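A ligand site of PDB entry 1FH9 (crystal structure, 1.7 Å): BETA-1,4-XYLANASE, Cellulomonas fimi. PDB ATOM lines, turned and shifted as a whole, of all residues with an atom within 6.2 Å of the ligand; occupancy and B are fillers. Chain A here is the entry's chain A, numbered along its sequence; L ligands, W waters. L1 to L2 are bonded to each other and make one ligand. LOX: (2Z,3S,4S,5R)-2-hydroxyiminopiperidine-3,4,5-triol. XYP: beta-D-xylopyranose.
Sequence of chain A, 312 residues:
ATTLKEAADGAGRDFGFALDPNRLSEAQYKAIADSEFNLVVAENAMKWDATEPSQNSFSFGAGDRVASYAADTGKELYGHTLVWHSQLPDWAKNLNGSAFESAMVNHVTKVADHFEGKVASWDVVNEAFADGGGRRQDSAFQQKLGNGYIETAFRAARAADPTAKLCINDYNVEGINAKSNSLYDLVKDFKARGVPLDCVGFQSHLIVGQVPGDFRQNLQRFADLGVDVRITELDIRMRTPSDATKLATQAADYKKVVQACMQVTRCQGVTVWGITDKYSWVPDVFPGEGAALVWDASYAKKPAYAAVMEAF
A ring nitrogen (NE2) of His 80 sits at hydrogen-bond distance from an oxygen (O3) of LOX L1, 2.6 Å away. The side-chain amide oxygen of Gln 203 sits at hydrogen-bond distance from an oxygen (ON1) of LOX L1 (2.7 Å). The side-chain carboxylate of Glu 127 lies within hydrogen-bond range of an oxygen (ON1) of LOX L1 (3.3 Å). An oxygen (O2) of XYP L2 is in hydrogen-bond range of the indole nitrogen of Trp 273. The side-chain carboxylate (OE2) of Glu 233 sits at hydrogen-bond distance from an oxygen (O2) of LOX L1 (2.6 Å). The side-chain amide nitrogen (ND2) of Asn 126 lies within hydrogen-bond range of an oxygen (O2) of LOX L1, 3.0 Å away. O5 of XYP L2 sits at hydrogen-bond distance from NZ of Lys 47. An oxygen (O3) of XYP L2 lies within hydrogen-bond range of the side-chain amide nitrogen (ND2) of Asn 44, at 2.9 Å. O5 of XYP L2 sits at hydrogen-bond distance from NE2 of Gln 87, 3.0 Å away. The side-chain carboxylate (OE2) of Glu 43 sits at hydrogen-bond distance from an oxygen (O2) of XYP L2 (2.7 Å). A ring nitrogen (NE2) of His 205 sits at hydrogen-bond distance from a nitrogen (N5) of LOX L1.
The backbone NH (N) of Glu 233 sits close to the backbone carbonyl oxygen (O) of Gln 203. The backbone carbonyl oxygen (O) of Glu 43 lies within hydrogen-bond range of the side-chain amino group (NZ) of Lys 47. NE2 of His 205 lies within hydrogen-bond range of OE1 of Glu 233. OE2 of Glu 233 sits at hydrogen-bond distance from ND2 of Asn 169. The side-chain amide nitrogen of Asn 169 lies close to the side-chain amide nitrogen of Gln 203, 2.7 Å away. OE1 of Glu 127 is in hydrogen-bond range of NE1 of Trp 84 (2.8 Å). The side-chain amide nitrogen (ND2) of Asn 126 sits close to the indole nitrogen (NE1) of Trp 84, at 3.2 Å. The side-chain amide oxygen of Asn 126 is in hydrogen-bond range of the side-chain amide nitrogen of Gln 203.
Trp 84 touches the ligand. Tyr 171 touches the ligand. CB of Trp 281 touches O2 of XYP L2 (3.4 Å). Hydrophobic or aromatic side chains that line the ligand: His 80, Trp 84, Tyr 171, His 205, Trp 273 and Trp 281. Within 4 Å of the ligand: Glu 43, Asn 44, Lys 47, His 80, Trp 84, Gln 87, Asn 126, Glu 127, Tyr 171, Gln 203, His 205, Glu 233, Trp 273 and Trp 281.
Water W4 bridges OG of Ser 86 (2.7 Å) and NE2 of Gln 87 (2.8 Å).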
ATOM      1  N   GLU A  43       8.977  -3.360   9.291  1.00  0.00           N
ATOM      2  CA  GLU A  43       8.185  -4.483   9.770  1.00  0.00           C
ATOM      3  C   GLU A  43       6.700  -4.162   9.691  1.00  0.00           C
ATOM      4  O   GLU A  43       5.895  -5.044   9.430  1.00  0.00           O
ATOM      5  CB  GLU A  43       8.566  -4.851  11.208  1.00  0.00           C
ATOM      6  CG  GLU A  43       7.671  -5.923  11.786  1.00  0.00           C
ATOM      7  CD  GLU A  43       8.007  -6.266  13.224  1.00  0.00           C
ATOM      8  OE1 GLU A  43       8.445  -5.351  13.954  1.00  0.00           O
ATOM      9  OE2 GLU A  43       7.793  -7.432  13.623  1.00  0.00           O
ATOM     10  N   ASN A  44       6.335  -2.886   9.894  1.00  0.00           N
ATOM     11  CA  ASN A  44       4.937  -2.469   9.854  1.00  0.00           C
ATOM     12  C   ASN A  44       4.687  -1.068   9.308  1.00  0.00           C
ATOM     13  O   ASN A  44       3.607  -0.783   8.794  1.00  0.00           O
ATOM     14  CB  ASN A  44       4.324  -2.535  11.261  1.00  0.00           C
ATOM     15  CG  ASN A  44       4.095  -3.953  11.739  1.00  0.00           C
ATOM     16  OD1 ASN A  44       3.319  -4.695  11.144  1.00  0.00           O
ATOM     17  ND2 ASN A  44       4.767  -4.322  12.832  1.00  0.00           N
ATOM     18  N   LYS A  47       2.896  -0.457   5.710  1.00  0.00           N
ATOM     19  CA  LYS A  47       1.713  -1.209   5.351  1.00  0.00           C
ATOM     20  C   LYS A  47       0.541  -0.251   5.172  1.00  0.00           C
ATOM     21  O   LYS A  47       0.622   0.922   5.548  1.00  0.00           O
ATOM     22  CB  LYS A  47       1.397  -2.239   6.447  1.00  0.00           C
ATOM     23  CG  LYS A  47       2.436  -3.340   6.530  1.00  0.00           C
ATOM     24  CD  LYS A  47       2.202  -4.243   7.730  1.00  0.00           C
ATOM     25  CE  LYS A  47       3.216  -5.384   7.731  1.00  0.00           C
ATOM     26  NZ  LYS A  47       3.105  -6.214   8.976  1.00  0.00           N
ATOM     27  N   HIS A  80       7.782  -3.024   2.173  1.00  0.00           N
ATOM     28  CA  HIS A  80       6.816  -4.053   2.513  1.00  0.00           C
ATOM     29  C   HIS A  80       5.608  -3.355   3.168  1.00  0.00           C
ATOM     30  O   HIS A  80       5.737  -2.770   4.215  1.00  0.00           O
ATOM     31  CB  HIS A  80       7.444  -5.058   3.515  1.00  0.00           C
ATOM     32  CG  HIS A  80       6.519  -6.168   3.954  1.00  0.00           C
ATOM     33  ND1 HIS A  80       6.230  -7.267   3.169  1.00  0.00           N
ATOM     34  CD2 HIS A  80       5.832  -6.358   5.116  1.00  0.00           C
ATOM     35  CE1 HIS A  80       5.406  -8.080   3.819  1.00  0.00           C
ATOM     36  NE2 HIS A  80       5.149  -7.550   4.997  1.00  0.00           N
ATOM     37  N   THR A  81       4.403  -3.374   2.597  1.00  0.00           N
ATOM     38  CA  THR A  81       3.967  -4.039   1.357  1.00  0.00           C
ATOM     39  C   THR A  81       2.743  -3.221   0.851  1.00  0.00           C
ATOM     40  O   THR A  81       1.854  -2.750   1.633  1.00  0.00           O
ATOM     41  CB  THR A  81       3.602  -5.572   1.624  1.00  0.00           C
ATOM     42  OG1 THR A  81       3.109  -6.219   0.405  1.00  0.00           O
ATOM     43  CG2 THR A  81       2.570  -5.678   2.764  1.00  0.00           C
ATOM     44  N   TRP A  84      -2.101  -5.980   0.338  1.00  0.00           N
ATOM     45  CA  TRP A  84      -2.107  -7.148   1.216  1.00  0.00           C
ATOM     46  C   TRP A  84      -3.493  -7.256   1.877  1.00  0.00           C
ATOM     47  O   TRP A  84      -4.060  -6.247   2.277  1.00  0.00           O
ATOM     48  CB  TRP A  84      -1.000  -7.029   2.272  1.00  0.00           C
ATOM     49  CG  TRP A  84      -0.819  -8.219   3.163  1.00  0.00           C
ATOM     50  CD1 TRP A  84      -1.019  -9.544   2.844  1.00  0.00           C
ATOM     51  CD2 TRP A  84      -0.327  -8.209   4.511  1.00  0.00           C
ATOM     52  NE1 TRP A  84      -0.684 -10.337   3.908  1.00  0.00           N
ATOM     53  CE2 TRP A  84      -0.251  -9.548   4.946  1.00  0.00           C
ATOM     54  CE3 TRP A  84       0.064  -7.190   5.390  1.00  0.00           C
ATOM     55  CZ2 TRP A  84       0.195  -9.901   6.228  1.00  0.00           C
ATOM     56  CZ3 TRP A  84       0.508  -7.531   6.665  1.00  0.00           C
ATOM     57  CH2 TRP A  84       0.569  -8.885   7.069  1.00  0.00           C
ATOM     58  N   SER A  86      -4.201  -8.481   4.742  1.00  0.00           N
ATOM     59  CA  SER A  86      -4.117  -8.255   6.187  1.00  0.00           C
ATOM     60  C   SER A  86      -3.707  -6.821   6.513  1.00  0.00           C
ATOM     61  O   SER A  86      -3.134  -6.118   5.672  1.00  0.00           O
ATOM     62  CB  SER A  86      -3.128  -9.251   6.797  1.00  0.00           C
ATOM     63  OG  SER A  86      -3.085  -9.115   8.209  1.00  0.00           O
ATOM     64  N   GLN A  87      -3.983  -6.392   7.740  1.00  0.00           N
ATOM     65  CA  GLN A  87      -3.681  -5.031   8.173  1.00  0.00           C
ATOM     66  C   GLN A  87      -4.221  -4.022   7.148  1.00  0.00           C
ATOM     67  O   GLN A  87      -3.553  -3.062   6.774  1.00  0.00           O
ATOM     68  CB  GLN A  87      -2.172  -4.859   8.407  1.00  0.00           C
ATOM     69  CG  GLN A  87      -1.712  -5.575   9.682  1.00  0.00           C
ATOM     70  CD  GLN A  87      -0.242  -5.403   9.982  1.00  0.00           C
ATOM     71  OE1 GLN A  87       0.201  -4.343  10.446  1.00  0.00           O
ATOM     72  NE2 GLN A  87       0.534  -6.445   9.727  1.00  0.00           N
ATOM     73  N   ASP A 123       7.340  -5.116  -2.235  1.00  0.00           N
ATOM     74  CA  ASP A 123       6.529  -6.333  -2.207  1.00  0.00           C
ATOM     75  C   ASP A 123       5.240  -5.654  -2.642  1.00  0.00           C
ATOM     76  O   ASP A 123       4.524  -5.095  -1.808  1.00  0.00           O
ATOM     77  CB  ASP A 123       6.340  -6.879  -0.791  1.00  0.00           C
ATOM     78  CG  ASP A 123       7.429  -7.839  -0.367  1.00  0.00           C
ATOM     79  OD1 ASP A 123       8.099  -8.423  -1.250  1.00  0.00           O
ATOM     80  OD2 ASP A 123       7.597  -8.013   0.859  1.00  0.00           O
ATOM     81  N   ASN A 126       1.244  -9.109  -1.661  1.00  0.00           N
ATOM     82  CA  ASN A 126       1.681 -10.041  -0.630  1.00  0.00           C
ATOM     83  C   ASN A 126       0.623 -11.111  -0.324  1.00  0.00           C
ATOM     84  O   ASN A 126      -0.557 -10.795  -0.182  1.00  0.00           O
ATOM     85  CB  ASN A 126       2.007  -9.245   0.635  1.00  0.00           C
ATOM     86  CG  ASN A 126       2.727 -10.062   1.698  1.00  0.00           C
ATOM     87  OD1 ASN A 126       3.593 -10.869   1.381  1.00  0.00           O
ATOM     88  ND2 ASN A 126       2.376  -9.841   2.959  1.00  0.00           N
ATOM     89  N   GLU A 127       1.065 -12.370  -0.239  1.00  0.00           N
ATOM     90  CA  GLU A 127       0.198 -13.516   0.088  1.00  0.00           C
ATOM     91  C   GLU A 127      -1.076 -13.662  -0.721  1.00  0.00           C
ATOM     92  O   GLU A 127      -2.170 -13.800  -0.160  1.00  0.00           O
ATOM     93  CB  GLU A 127      -0.154 -13.461   1.580  1.00  0.00           C
ATOM     94  CG  GLU A 127       1.048 -13.145   2.447  1.00  0.00           C
ATOM     95  CD  GLU A 127       0.757 -13.164   3.927  1.00  0.00           C
ATOM     96  OE1 GLU A 127      -0.421 -13.046   4.315  1.00  0.00           O
ATOM     97  OE2 GLU A 127       1.723 -13.293   4.702  1.00  0.00           O
ATOM     98  N   ASN A 169       5.291 -11.386  -3.071  1.00  0.00           N
ATOM     99  CA  ASN A 169       5.745 -12.086  -1.876  1.00  0.00           C
ATOM    100  C   ASN A 169       4.746 -13.111  -1.348  1.00  0.00           C
ATOM    101  O   ASN A 169       3.533 -12.921  -1.481  1.00  0.00           O
ATOM    102  CB  ASN A 169       6.049 -11.034  -0.789  1.00  0.00           C
ATOM    103  CG  ASN A 169       6.933 -11.570   0.323  1.00  0.00           C
ATOM    104  OD1 ASN A 169       7.940 -12.225   0.060  1.00  0.00           O
ATOM    105  ND2 ASN A 169       6.574 -11.272   1.561  1.00  0.00           N
ATOM    106  N   TYR A 171       4.369 -16.897   1.588  1.00  0.00           N
ATOM    107  CA  TYR A 171       4.983 -17.843   2.515  1.00  0.00           C
ATOM    108  C   TYR A 171       4.572 -19.265   2.167  1.00  0.00           C
ATOM    109  O   TYR A 171       3.597 -19.472   1.445  1.00  0.00           O
ATOM    110  CB  TYR A 171       4.582 -17.495   3.947  1.00  0.00           C
ATOM    111  CG  TYR A 171       3.103 -17.633   4.252  1.00  0.00           C
ATOM    112  CD1 TYR A 171       2.554 -18.866   4.618  1.00  0.00           C
ATOM    113  CD2 TYR A 171       2.255 -16.535   4.197  1.00  0.00           C
ATOM    114  CE1 TYR A 171       1.192 -18.990   4.933  1.00  0.00           C
ATOM    115  CE2 TYR A 171       0.903 -16.652   4.506  1.00  0.00           C
ATOM    116  CZ  TYR A 171       0.375 -17.870   4.874  1.00  0.00           C
ATOM    117  OH  TYR A 171      -0.965 -17.970   5.192  1.00  0.00           O
ATOM    118  N   GLN A 203       9.160 -15.461   1.817  1.00  0.00           N
ATOM    119  CA  GLN A 203       9.125 -15.088   3.235  1.00  0.00           C
ATOM    120  C   GLN A 203       9.942 -15.995   4.142  1.00  0.00           C
ATOM    121  O   GLN A 203      10.678 -15.523   5.005  1.00  0.00           O
ATOM    122  CB  GLN A 203       7.658 -15.013   3.690  1.00  0.00           C
ATOM    123  CG  GLN A 203       6.970 -13.781   3.119  1.00  0.00           C
ATOM    124  CD  GLN A 203       5.490 -13.738   3.387  1.00  0.00           C
ATOM    125  OE1 GLN A 203       4.987 -14.351   4.316  1.00  0.00           O
ATOM    126  NE2 GLN A 203       4.769 -12.972   2.575  1.00  0.00           N
ATOM    127  N   HIS A 205       9.094 -18.205   6.648  1.00  0.00           N
ATOM    128  CA  HIS A 205       8.763 -18.282   8.066  1.00  0.00           C
ATOM    129  C   HIS A 205       8.712 -19.791   8.256  1.00  0.00           C
ATOM    130  O   HIS A 205       7.664 -20.415   8.086  1.00  0.00           O
ATOM    131  CB  HIS A 205       7.405 -17.636   8.336  1.00  0.00           C
ATOM    132  CG  HIS A 205       7.444 -16.139   8.302  1.00  0.00           C
ATOM    133  ND1 HIS A 205       8.155 -15.385   9.208  1.00  0.00           N
ATOM    134  CD2 HIS A 205       6.861 -15.248   7.451  1.00  0.00           C
ATOM    135  CE1 HIS A 205       8.014 -14.104   8.929  1.00  0.00           C
ATOM    136  NE2 HIS A 205       7.228 -13.993   7.859  1.00  0.00           N
ATOM    137  N   GLU A 233      11.455 -12.696   4.823  1.00  0.00           N
ATOM    138  CA  GLU A 233      11.045 -12.608   6.228  1.00  0.00           C
ATOM    139  C   GLU A 233      11.481 -13.817   7.034  1.00  0.00           C
ATOM    140  O   GLU A 233      10.707 -14.417   7.781  1.00  0.00           O
ATOM    141  CB  GLU A 233       9.527 -12.450   6.303  1.00  0.00           C
ATOM    142  CG  GLU A 233       8.960 -11.363   5.394  1.00  0.00           C
ATOM    143  CD  GLU A 233       7.454 -11.273   5.479  1.00  0.00           C
ATOM    144  OE1 GLU A 233       6.888 -11.835   6.441  1.00  0.00           O
ATOM    145  OE2 GLU A 233       6.826 -10.631   4.617  1.00  0.00           O
ATOM    146  N   TRP A 273      13.177 -11.514   9.711  1.00  0.00           N
ATOM    147  CA  TRP A 273      12.054 -10.734  10.227  1.00  0.00           C
ATOM    148  C   TRP A 273      12.247 -10.258  11.663  1.00  0.00           C
ATOM    149  O   TRP A 273      11.489 -10.637  12.560  1.00  0.00           O
ATOM    150  CB  TRP A 273      10.754 -11.529  10.102  1.00  0.00           C
ATOM    151  CG  TRP A 273       9.571 -10.632   9.965  1.00  0.00           C
ATOM    152  CD1 TRP A 273       8.511 -10.539  10.827  1.00  0.00           C
ATOM    153  CD2 TRP A 273       9.353  -9.678   8.937  1.00  0.00           C
ATOM    154  NE1 TRP A 273       7.647  -9.569  10.385  1.00  0.00           N
ATOM    155  CE2 TRP A 273       8.133  -9.016   9.226  1.00  0.00           C
ATOM    156  CE3 TRP A 273      10.059  -9.293   7.790  1.00  0.00           C
ATOM    157  CZ2 TRP A 273       7.610  -7.999   8.418  1.00  0.00           C
ATOM    158  CZ3 TRP A 273       9.535  -8.277   6.981  1.00  0.00           C
ATOM    159  CH2 TRP A 273       8.321  -7.650   7.307  1.00  0.00           C
ATOM    160  N   TRP A 281       7.705 -11.401  16.281  1.00  0.00           N
ATOM    161  CA  TRP A 281       6.259 -11.504  16.183  1.00  0.00           C
ATOM    162  C   TRP A 281       5.694 -12.906  16.427  1.00  0.00           C
ATOM    163  O   TRP A 281       4.496 -13.072  16.651  1.00  0.00           O
ATOM    164  CB  TRP A 281       5.809 -11.061  14.778  1.00  0.00           C
ATOM    165  CG  TRP A 281       6.104 -12.093  13.711  1.00  0.00           C
ATOM    166  CD1 TRP A 281       7.321 -12.593  13.355  1.00  0.00           C
ATOM    167  CD2 TRP A 281       5.143 -12.754  12.868  1.00  0.00           C
ATOM    168  NE1 TRP A 281       7.188 -13.526  12.355  1.00  0.00           N
ATOM    169  CE2 TRP A 281       5.857 -13.650  12.045  1.00  0.00           C
ATOM    170  CE3 TRP A 281       3.748 -12.694  12.754  1.00  0.00           C
ATOM    171  CZ2 TRP A 281       5.226 -14.471  11.101  1.00  0.00           C
ATOM    172  CZ3 TRP A 281       3.120 -13.505  11.811  1.00  0.00           C
ATOM    173  CH2 TRP A 281       3.861 -14.379  10.999  1.00  0.00           C
ATOM    174  N   VAL A 285       1.548 -14.846  17.775  1.00  0.00           N
ATOM    175  CA  VAL A 285       0.794 -15.377  16.646  1.00  0.00           C
ATOM    176  C   VAL A 285       0.775 -16.900  16.633  1.00  0.00           C
ATOM    177  O   VAL A 285      -0.192 -17.520  16.182  1.00  0.00           O
ATOM    178  CB  VAL A 285       1.382 -14.872  15.302  1.00  0.00           C
ATOM    179  CG1 VAL A 285       0.646 -15.523  14.126  1.00  0.00           C
ATOM    180  CG2 VAL A 285       1.283 -13.358  15.219  1.00  0.00           C
HETATM  181  C1  LOX L   1       3.959 -12.212   6.979  1.00  0.00           C
HETATM  182  C2  LOX L   1       3.770 -10.737   6.448  1.00  0.00           C
HETATM  183  C3  LOX L   1       4.444  -9.700   7.445  1.00  0.00           C
HETATM  184  C4  LOX L   1       4.157 -10.089   8.909  1.00  0.00           C
HETATM  185  C5  LOX L   1       4.901 -11.406   9.267  1.00  0.00           C
HETATM  186  N5  LOX L   1       4.464 -12.428   8.282  1.00  0.00           N
HETATM  187  ON1 LOX L   1       3.991 -14.435   6.853  1.00  0.00           O
HETATM  188  N1  LOX L   1       3.684 -13.276   6.231  1.00  0.00           N
HETATM  189  O2  LOX L   1       4.250 -10.547   5.156  1.00  0.00           O
HETATM  190  O3  LOX L   1       3.942  -8.374   7.207  1.00  0.00           O
HETATM  191  O4  LOX L   1       4.634  -9.066   9.779  1.00  0.00           O
HETATM  192  C1  XYP L   2       3.841  -9.012  10.994  1.00  0.00           C
HETATM  193  C2  XYP L   2       4.560  -8.106  11.999  1.00  0.00           C
HETATM  194  C3  XYP L   2       3.692  -7.902  13.244  1.00  0.00           C
HETATM  195  C4  XYP L   2       2.289  -7.429  12.860  1.00  0.00           C
HETATM  196  C5  XYP L   2       1.684  -8.371  11.814  1.00  0.00           C
HETATM  197  O2  XYP L   2       5.790  -8.700  12.360  1.00  0.00           O
HETATM  198  O3  XYP L   2       4.299  -6.932  14.083  1.00  0.00           O
HETATM  199  O4  XYP L   2       1.471  -7.385  14.014  1.00  0.00           O
HETATM  200  O5  XYP L   2       2.550  -8.473  10.660  1.00  0.00           O
HETATM  201  O   HOH W   1       4.535  -8.073  16.667  1.00  0.00           O
HETATM  202  O   HOH W   2       1.220 -10.136  15.099  1.00  0.00           O
HETATM  203  O   HOH W   3       1.874 -15.238   7.855  1.00  0.00           O
HETATM  204  O   HOH W   4      -1.009  -8.793   9.865  1.00  0.00           O
